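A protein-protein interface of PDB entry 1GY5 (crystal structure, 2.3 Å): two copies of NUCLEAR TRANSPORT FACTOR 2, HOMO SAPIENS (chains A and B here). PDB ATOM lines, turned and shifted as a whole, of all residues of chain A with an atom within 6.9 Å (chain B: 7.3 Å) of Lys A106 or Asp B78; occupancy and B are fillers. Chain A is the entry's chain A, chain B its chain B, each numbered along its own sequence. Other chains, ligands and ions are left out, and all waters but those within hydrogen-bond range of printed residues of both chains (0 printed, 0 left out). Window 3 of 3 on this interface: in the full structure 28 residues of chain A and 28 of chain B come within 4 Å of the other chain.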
ATOM      1  N   ILE A  34     -29.165  12.587  -9.041  1.00  0.00           N
ATOM      2  CA  ILE A  34     -29.830  12.566  -7.747  1.00  0.00           C
ATOM      3  C   ILE A  34     -31.098  13.398  -7.926  1.00  0.00           C
ATOM      4  O   ILE A  34     -31.372  13.860  -9.035  1.00  0.00           O
ATOM      5  CB  ILE A  34     -28.938  13.143  -6.626  1.00  0.00           C
ATOM      6  CG1 ILE A  34     -28.496  14.566  -6.971  1.00  0.00           C
ATOM      7  CG2 ILE A  34     -27.737  12.240  -6.418  1.00  0.00           C
ATOM      8  CD1 ILE A  34     -27.685  15.245  -5.886  1.00  0.00           C
ATOM      9  N   THR A  76     -13.946  23.407  -8.241  1.00  0.00           N
ATOM     10  CA  THR A  76     -14.681  24.587  -7.778  1.00  0.00           C
ATOM     11  C   THR A  76     -14.383  24.813  -6.303  1.00  0.00           C
ATOM     12  O   THR A  76     -13.916  23.906  -5.604  1.00  0.00           O
ATOM     13  CB  THR A  76     -16.226  24.447  -7.932  1.00  0.00           C
ATOM     14  OG1 THR A  76     -16.719  23.555  -6.934  1.00  0.00           O
ATOM     15  CG2 THR A  76     -16.603  23.907  -9.310  1.00  0.00           C
ATOM     16  N   ASP A  78     -16.222  24.871  -3.787  1.00  0.00           N
ATOM     17  CA  ASP A  78     -16.907  23.874  -2.963  1.00  0.00           C
ATOM     18  C   ASP A  78     -16.477  22.437  -3.249  1.00  0.00           C
ATOM     19  O   ASP A  78     -17.134  21.489  -2.825  1.00  0.00           O
ATOM     20  CB  ASP A  78     -18.424  24.011  -3.117  1.00  0.00           C
ATOM     21  CG  ASP A  78     -18.976  25.226  -2.377  1.00  0.00           C
ATOM     22  OD1 ASP A  78     -18.905  25.244  -1.131  1.00  0.00           O
ATOM     23  OD2 ASP A  78     -19.475  26.167  -3.041  1.00  0.00           O
ATOM     24  N   SER A  79     -15.367  22.280  -3.965  1.00  0.00           N
ATOM     25  CA  SER A  79     -14.827  20.966  -4.287  1.00  0.00           C
ATOM     26  C   SER A  79     -15.673  20.133  -5.251  1.00  0.00           C
ATOM     27  O   SER A  79     -15.738  18.910  -5.144  1.00  0.00           O
ATOM     28  CB  SER A  79     -14.582  20.178  -3.004  1.00  0.00           C
ATOM     29  OG  SER A  79     -13.722  20.890  -2.132  1.00  0.00           O
ATOM     30  N   CYS A  80     -16.343  20.811  -6.177  1.00  0.00           N
ATOM     31  CA  CYS A  80     -17.129  20.139  -7.201  1.00  0.00           C
ATOM     32  C   CYS A  80     -16.212  20.155  -8.420  1.00  0.00           C
ATOM     33  O   CYS A  80     -15.157  20.809  -8.408  1.00  0.00           O
ATOM     34  CB  CYS A  80     -18.405  20.924  -7.524  1.00  0.00           C
ATOM     35  SG  CYS A  80     -19.678  20.874  -6.240  1.00  0.00           S
ATOM     36  N   ILE A  81     -16.594  19.434  -9.465  1.00  0.00           N
ATOM     37  CA  ILE A  81     -15.800  19.437 -10.677  1.00  0.00           C
ATOM     38  C   ILE A  81     -16.709  19.853 -11.815  1.00  0.00           C
ATOM     39  O   ILE A  81     -17.808  19.335 -11.969  1.00  0.00           O
ATOM     40  CB  ILE A  81     -15.196  18.058 -10.995  1.00  0.00           C
ATOM     41  CG1 ILE A  81     -14.230  17.640  -9.881  1.00  0.00           C
ATOM     42  CG2 ILE A  81     -14.432  18.126 -12.321  1.00  0.00           C
ATOM     43  CD1 ILE A  81     -13.745  16.214 -10.001  1.00  0.00           C
ATOM     44  N   LEU A 104     -21.615  19.263 -14.077  1.00  0.00           N
ATOM     45  CA  LEU A 104     -21.088  19.738 -12.808  1.00  0.00           C
ATOM     46  C   LEU A 104     -21.150  18.497 -11.920  1.00  0.00           C
ATOM     47  O   LEU A 104     -22.202  17.878 -11.786  1.00  0.00           O
ATOM     48  CB  LEU A 104     -21.937  20.865 -12.218  1.00  0.00           C
ATOM     49  CG  LEU A 104     -21.354  21.360 -10.888  1.00  0.00           C
ATOM     50  CD1 LEU A 104     -19.975  21.950 -11.131  1.00  0.00           C
ATOM     51  CD2 LEU A 104     -22.283  22.391 -10.244  1.00  0.00           C
ATOM     52  N   LEU A 105     -20.023  18.114 -11.334  1.00  0.00           N
ATOM     53  CA  LEU A 105     -19.999  16.923 -10.503  1.00  0.00           C
ATOM     54  C   LEU A 105     -19.763  17.242  -9.039  1.00  0.00           C
ATOM     55  O   LEU A 105     -18.987  18.135  -8.701  1.00  0.00           O
ATOM     56  CB  LEU A 105     -18.915  15.966 -10.995  1.00  0.00           C
ATOM     57  CG  LEU A 105     -18.831  15.707 -12.502  1.00  0.00           C
ATOM     58  CD1 LEU A 105     -17.542  14.967 -12.812  1.00  0.00           C
ATOM     59  CD2 LEU A 105     -20.056  14.913 -12.971  1.00  0.00           C
ATOM     60  N   LYS A 106     -20.439  16.495  -8.175  1.00  0.00           N
ATOM     61  CA  LYS A 106     -20.300  16.667  -6.740  1.00  0.00           C
ATOM     62  C   LYS A 106     -20.162  15.299  -6.081  1.00  0.00           C
ATOM     63  O   LYS A 106     -20.798  14.334  -6.506  1.00  0.00           O
ATOM     64  CB  LYS A 106     -21.520  17.398  -6.169  1.00  0.00           C
ATOM     65  CG  LYS A 106     -21.395  17.689  -4.684  1.00  0.00           C
ATOM     66  CD  LYS A 106     -22.543  18.539  -4.160  1.00  0.00           C
ATOM     67  CE  LYS A 106     -22.335  18.877  -2.686  1.00  0.00           C
ATOM     68  NZ  LYS A 106     -23.497  19.621  -2.115  1.00  0.00           N
ATOM     69  N   ASN A 107     -19.325  15.206  -5.051  1.00  0.00           N
ATOM     70  CA  ASN A 107     -19.151  13.934  -4.362  1.00  0.00           C
ATOM     71  C   ASN A 107     -20.093  13.834  -3.162  1.00  0.00           C
ATOM     72  O   ASN A 107     -19.951  14.566  -2.184  1.00  0.00           O
ATOM     73  CB  ASN A 107     -17.710  13.758  -3.884  1.00  0.00           C
ATOM     74  CG  ASN A 107     -17.499  12.434  -3.162  1.00  0.00           C
ATOM     75  OD1 ASN A 107     -16.869  11.519  -3.692  1.00  0.00           O
ATOM     76  ND2 ASN A 107     -18.043  12.323  -1.955  1.00  0.00           N
ATOM     77  N   ILE A 108     -21.051  12.921  -3.249  1.00  0.00           N
ATOM     78  CA  ILE A 108     -22.028  12.698  -2.189  1.00  0.00           C
ATOM     79  C   ILE A 108     -21.990  11.233  -1.768  1.00  0.00           C
ATOM     80  O   ILE A 108     -21.840  10.346  -2.609  1.00  0.00           O
ATOM     81  CB  ILE A 108     -23.440  13.040  -2.673  1.00  0.00           C
ATOM     82  CG1 ILE A 108     -23.578  14.553  -2.819  1.00  0.00           C
ATOM     83  CG2 ILE A 108     -24.476  12.471  -1.719  1.00  0.00           C
ATOM     84  CD1 ILE A 108     -24.970  14.999  -3.192  1.00  0.00           C
ATOM     85  N   ALA A 111     -19.430   9.365  -3.342  1.00  0.00           N
ATOM     86  CA  ALA A 111     -19.537   8.927  -4.734  1.00  0.00           C
ATOM     87  C   ALA A 111     -19.750  10.150  -5.622  1.00  0.00           C
ATOM     88  O   ALA A 111     -20.385  11.124  -5.207  1.00  0.00           O
ATOM     89  CB  ALA A 111     -20.705   7.952  -4.898  1.00  0.00           C
ATOM     90  N   TRP A 112     -19.220  10.110  -6.839  1.00  0.00           N
ATOM     91  CA  TRP A 112     -19.396  11.241  -7.733  1.00  0.00           C
ATOM     92  C   TRP A 112     -20.706  11.159  -8.504  1.00  0.00           C
ATOM     93  O   TRP A 112     -20.951  10.205  -9.241  1.00  0.00           O
ATOM     94  CB  TRP A 112     -18.225  11.355  -8.716  1.00  0.00           C
ATOM     95  CG  TRP A 112     -16.954  11.819  -8.070  1.00  0.00           C
ATOM     96  CD1 TRP A 112     -15.896  11.046  -7.695  1.00  0.00           C
ATOM     97  CD2 TRP A 112     -16.631  13.161  -7.668  1.00  0.00           C
ATOM     98  NE1 TRP A 112     -14.938  11.819  -7.083  1.00  0.00           N
ATOM     99  CE2 TRP A 112     -15.364  13.119  -7.054  1.00  0.00           C
ATOM    100  CE3 TRP A 112     -17.292  14.392  -7.767  1.00  0.00           C
ATOM    101  CZ2 TRP A 112     -14.743  14.264  -6.538  1.00  0.00           C
ATOM    102  CZ3 TRP A 112     -16.675  15.530  -7.252  1.00  0.00           C
ATOM    103  CH2 TRP A 112     -15.417  15.456  -6.648  1.00  0.00           C
ATOM    104  N   VAL A 113     -21.551  12.166  -8.314  1.00  0.00           N
ATOM    105  CA  VAL A 113     -22.825  12.235  -9.010  1.00  0.00           C
ATOM    106  C   VAL A 113     -22.855  13.522  -9.818  1.00  0.00           C
ATOM    107  O   VAL A 113     -22.081  14.442  -9.559  1.00  0.00           O
ATOM    108  CB  VAL A 113     -24.013  12.256  -8.031  1.00  0.00           C
ATOM    109  CG1 VAL A 113     -23.987  11.014  -7.159  1.00  0.00           C
ATOM    110  CG2 VAL A 113     -23.968  13.526  -7.180  1.00  0.00           C
ATOM    111  N   CYS A 114     -23.745  13.584 -10.801  1.00  0.00           N
ATOM    112  CA  CYS A 114     -23.874  14.783 -11.622  1.00  0.00           C
ATOM    113  C   CYS A 114     -25.084  15.594 -11.151  1.00  0.00           C
ATOM    114  O   CYS A 114     -26.219  15.125 -11.215  1.00  0.00           O
ATOM    115  CB  CYS A 114     -24.048  14.399 -13.081  1.00  0.00           C
ATOM    116  SG  CYS A 114     -24.435  15.785 -14.140  1.00  0.00           S
ATOM    117  N   THR A 115     -24.836  16.807 -10.663  1.00  0.00           N
ATOM    118  CA  THR A 115     -25.913  17.668 -10.177  1.00  0.00           C
ATOM    119  C   THR A 115     -26.481  18.582 -11.269  1.00  0.00           C
ATOM    120  O   THR A 115     -27.627  19.006 -11.185  1.00  0.00           O
ATOM    121  CB  THR A 115     -25.431  18.568  -9.016  1.00  0.00           C
ATOM    122  OG1 THR A 115     -24.379  19.422  -9.483  1.00  0.00           O
ATOM    123  CG2 THR A 115     -24.935  17.720  -7.846  1.00  0.00           C
ATOM    124  N   PRO B  75     -29.822  26.074 -11.181  1.00  0.00           N
ATOM    125  CA  PRO B  75     -29.336  26.311  -9.820  1.00  0.00           C
ATOM    126  C   PRO B  75     -28.531  25.064  -9.421  1.00  0.00           C
ATOM    127  O   PRO B  75     -28.767  23.979  -9.961  1.00  0.00           O
ATOM    128  CB  PRO B  75     -30.624  26.424  -9.022  1.00  0.00           C
ATOM    129  CG  PRO B  75     -31.469  25.340  -9.666  1.00  0.00           C
ATOM    130  CD  PRO B  75     -31.206  25.550 -11.161  1.00  0.00           C
ATOM    131  N   THR B  76     -27.586  25.197  -8.494  1.00  0.00           N
ATOM    132  CA  THR B  76     -26.826  24.024  -8.065  1.00  0.00           C
ATOM    133  C   THR B  76     -27.175  23.757  -6.603  1.00  0.00           C
ATOM    134  O   THR B  76     -27.620  24.653  -5.895  1.00  0.00           O
ATOM    135  CB  THR B  76     -25.310  24.236  -8.201  1.00  0.00           C
ATOM    136  OG1 THR B  76     -24.858  25.144  -7.184  1.00  0.00           O
ATOM    137  CG2 THR B  76     -24.977  24.801  -9.577  1.00  0.00           C
ATOM    138  N   PRO B  77     -26.985  22.519  -6.134  1.00  0.00           N
ATOM    139  CA  PRO B  77     -27.304  22.193  -4.740  1.00  0.00           C
ATOM    140  C   PRO B  77     -26.622  23.106  -3.715  1.00  0.00           C
ATOM    141  O   PRO B  77     -27.148  23.317  -2.620  1.00  0.00           O
ATOM    142  CB  PRO B  77     -26.847  20.740  -4.611  1.00  0.00           C
ATOM    143  CG  PRO B  77     -27.015  20.204  -5.990  1.00  0.00           C
ATOM    144  CD  PRO B  77     -26.489  21.331  -6.850  1.00  0.00           C
ATOM    145  N   ASP B  78     -25.453  23.636  -4.070  1.00  0.00           N
ATOM    146  CA  ASP B  78     -24.702  24.509  -3.174  1.00  0.00           C
ATOM    147  C   ASP B  78     -25.120  25.974  -3.302  1.00  0.00           C
ATOM    148  O   ASP B  78     -24.364  26.883  -2.950  1.00  0.00           O
ATOM    149  CB  ASP B  78     -23.199  24.369  -3.434  1.00  0.00           C
ATOM    150  CG  ASP B  78     -22.680  22.969  -3.128  1.00  0.00           C
ATOM    151  OD1 ASP B  78     -22.957  22.466  -2.018  1.00  0.00           O
ATOM    152  OD2 ASP B  78     -21.991  22.371  -3.986  1.00  0.00           O
ATOM    153  N   SER B  79     -26.326  26.193  -3.805  1.00  0.00           N
ATOM    154  CA  SER B  79     -26.867  27.537  -3.966  1.00  0.00           C
ATOM    155  C   SER B  79     -26.117  28.380  -4.985  1.00  0.00           C
ATOM    156  O   SER B  79     -26.153  29.603  -4.920  1.00  0.00           O
ATOM    157  CB  SER B  79     -26.883  28.265  -2.622  1.00  0.00           C
ATOM    158  OG  SER B  79     -27.515  27.471  -1.637  1.00  0.00           O
ATOM    159  N   CYS B  80     -25.428  27.720  -5.908  1.00  0.00           N
ATOM    160  CA  CYS B  80     -24.702  28.416  -6.965  1.00  0.00           C
ATOM    161  C   CYS B  80     -25.571  28.418  -8.226  1.00  0.00           C
ATOM    162  O   CYS B  80     -26.643  27.810  -8.269  1.00  0.00           O
ATOM    163  CB  CYS B  80     -23.372  27.712  -7.276  1.00  0.00           C
ATOM    164  SG  CYS B  80     -22.106  27.833  -5.987  1.00  0.00           S
ATOM    165  N   ILE B  81     -25.095  29.093  -9.260  1.00  0.00           N
ATOM    166  CA  ILE B  81     -25.819  29.157 -10.517  1.00  0.00           C
ATOM    167  C   ILE B  81     -24.860  28.891 -11.686  1.00  0.00           C
ATOM    168  O   ILE B  81     -23.755  29.438 -11.739  1.00  0.00           O
ATOM    169  CB  ILE B  81     -26.494  30.545 -10.685  1.00  0.00           C
ATOM    170  CG1 ILE B  81     -27.499  30.766  -9.538  1.00  0.00           C
ATOM    171  CG2 ILE B  81     -27.168  30.647 -12.050  1.00  0.00           C
ATOM    172  CD1 ILE B  81     -28.330  32.041  -9.669  1.00  0.00           C
ATOM    173  N   LEU B 105     -21.538  30.811 -10.957  1.00  0.00           N
ATOM    174  CA  LEU B 105     -21.671  31.995 -10.116  1.00  0.00           C
ATOM    175  C   LEU B 105     -21.991  31.642  -8.672  1.00  0.00           C
ATOM    176  O   LEU B 105     -22.757  30.715  -8.396  1.00  0.00           O
ATOM    177  CB  LEU B 105     -22.782  32.896 -10.662  1.00  0.00           C
ATOM    178  CG  LEU B 105     -22.761  33.204 -12.156  1.00  0.00           C
ATOM    179  CD1 LEU B 105     -24.002  34.013 -12.517  1.00  0.00           C
ATOM    180  CD2 LEU B 105     -21.475  33.959 -12.518  1.00  0.00           C
ATOM    181  N   LYS B 106     -21.398  32.396  -7.756  1.00  0.00           N
ATOM    182  CA  LYS B 106     -21.615  32.196  -6.334  1.00  0.00           C
ATOM    183  C   LYS B 106     -21.852  33.559  -5.691  1.00  0.00           C
ATOM    184  O   LYS B 106     -21.183  34.535  -6.025  1.00  0.00           O
ATOM    185  CB  LYS B 106     -20.396  31.523  -5.697  1.00  0.00           C
ATOM    186  CG  LYS B 106     -20.552  31.228  -4.214  1.00  0.00           C
ATOM    187  CD  LYS B 106     -19.310  30.554  -3.653  1.00  0.00           C
ATOM    188  CE  LYS B 106     -19.472  30.237  -2.176  1.00  0.00           C
ATOM    189  NZ  LYS B 106     -20.620  29.323  -1.927  1.00  0.00           N
ATOM    190  N   ASN B 107     -22.812  33.612  -4.775  1.00  0.00           N
ATOM    191  CA  ASN B 107     -23.159  34.842  -4.071  1.00  0.00           C
ATOM    192  C   ASN B 107     -22.189  35.082  -2.914  1.00  0.00           C
ATOM    193  O   ASN B 107     -22.079  34.267  -2.005  1.00  0.00           O
ATOM    194  CB  ASN B 107     -24.587  34.734  -3.527  1.00  0.00           C
ATOM    195  CG  ASN B 107     -25.138  36.064  -3.063  1.00  0.00           C
ATOM    196  OD1 ASN B 107     -24.514  36.765  -2.274  1.00  0.00           O
ATOM    197  ND2 ASN B 107     -26.321  36.415  -3.554  1.00  0.00           N
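The side-chain carboxylate (OD2) of Asp A78 lies within salt-bridge range of the side-chain amino group (NZ) of Lys B106.
SG of Cys A80 is in hydrogen-bond range of OD2 of Asp B78.
The side-chain amino group (NZ) of Lys A106 lies within salt-bridge range of the side-chain carboxylate (OD1) of Asp B78.
The side-chain hydroxyl (OG1) of Thr B76 is in hydrogen-bond range of the backbone NH (N) of Cys B80 (2.9 Å).
OG1 of Thr A76 is in hydrogen-bond range of N of Cys A80 (2.9 Å).
The side-chain sulfur (SG) of Cys A80 lies close to the backbone carbonyl oxygen (O) of Leu A105 (3.7 Å).
The backbone carbonyl oxygen (O) of Lys A106 sits at hydrogen-bond distance from the backbone NH (N) of Val A113, 2.9 Å away.
The backbone NH (N) of Asp A78 lies close to the side-chain hydroxyl (OG1) of Thr A76, 3.4 Å away.
The backbone NH (N) of Thr A115 lies within hydrogen-bond range of the backbone carbonyl oxygen (O) of Leu A104 (3.1 Å).
Thr B76 touches Leu A104.
Thr A115 touches Pro B77 (CB to CD, 3.7 Å).
Of chain B, only Asp B78 (2.9 Å) comes within 4 Å of Lys A106.
Printed residues of chain B within 4 Å of Asp A78: Lys B106 (3.5 Å).
Of the printed residues of chain B, Cys A80 touches Asp B78 (3.6 Å).
Asn B107 touches none of the printed residues of chain A.
The nearest residue of chain B that does not touch Lys A106 is Pro B77 (4.3 Å).
The nearest residue of chain A that does not touch Asp B78 is Asp A78 (4.02 Å).
Hydrophobic or aromatic side chains of chain B within 4 Å of the printed part of chain A: Pro B77.
Asp A78 touches Lys B106, and with the chains exchanged Lys A106 touches Asp B78.
Cys A80 touches Asp B78, but with the chains exchanged Asp A78 does not touch Cys B80 (4.3 Å).
8 positions are printed for both chains.
Of the 5 pairs that touch across the chains among the printed residues, 2 have their exchanged pair printed and touching as well.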
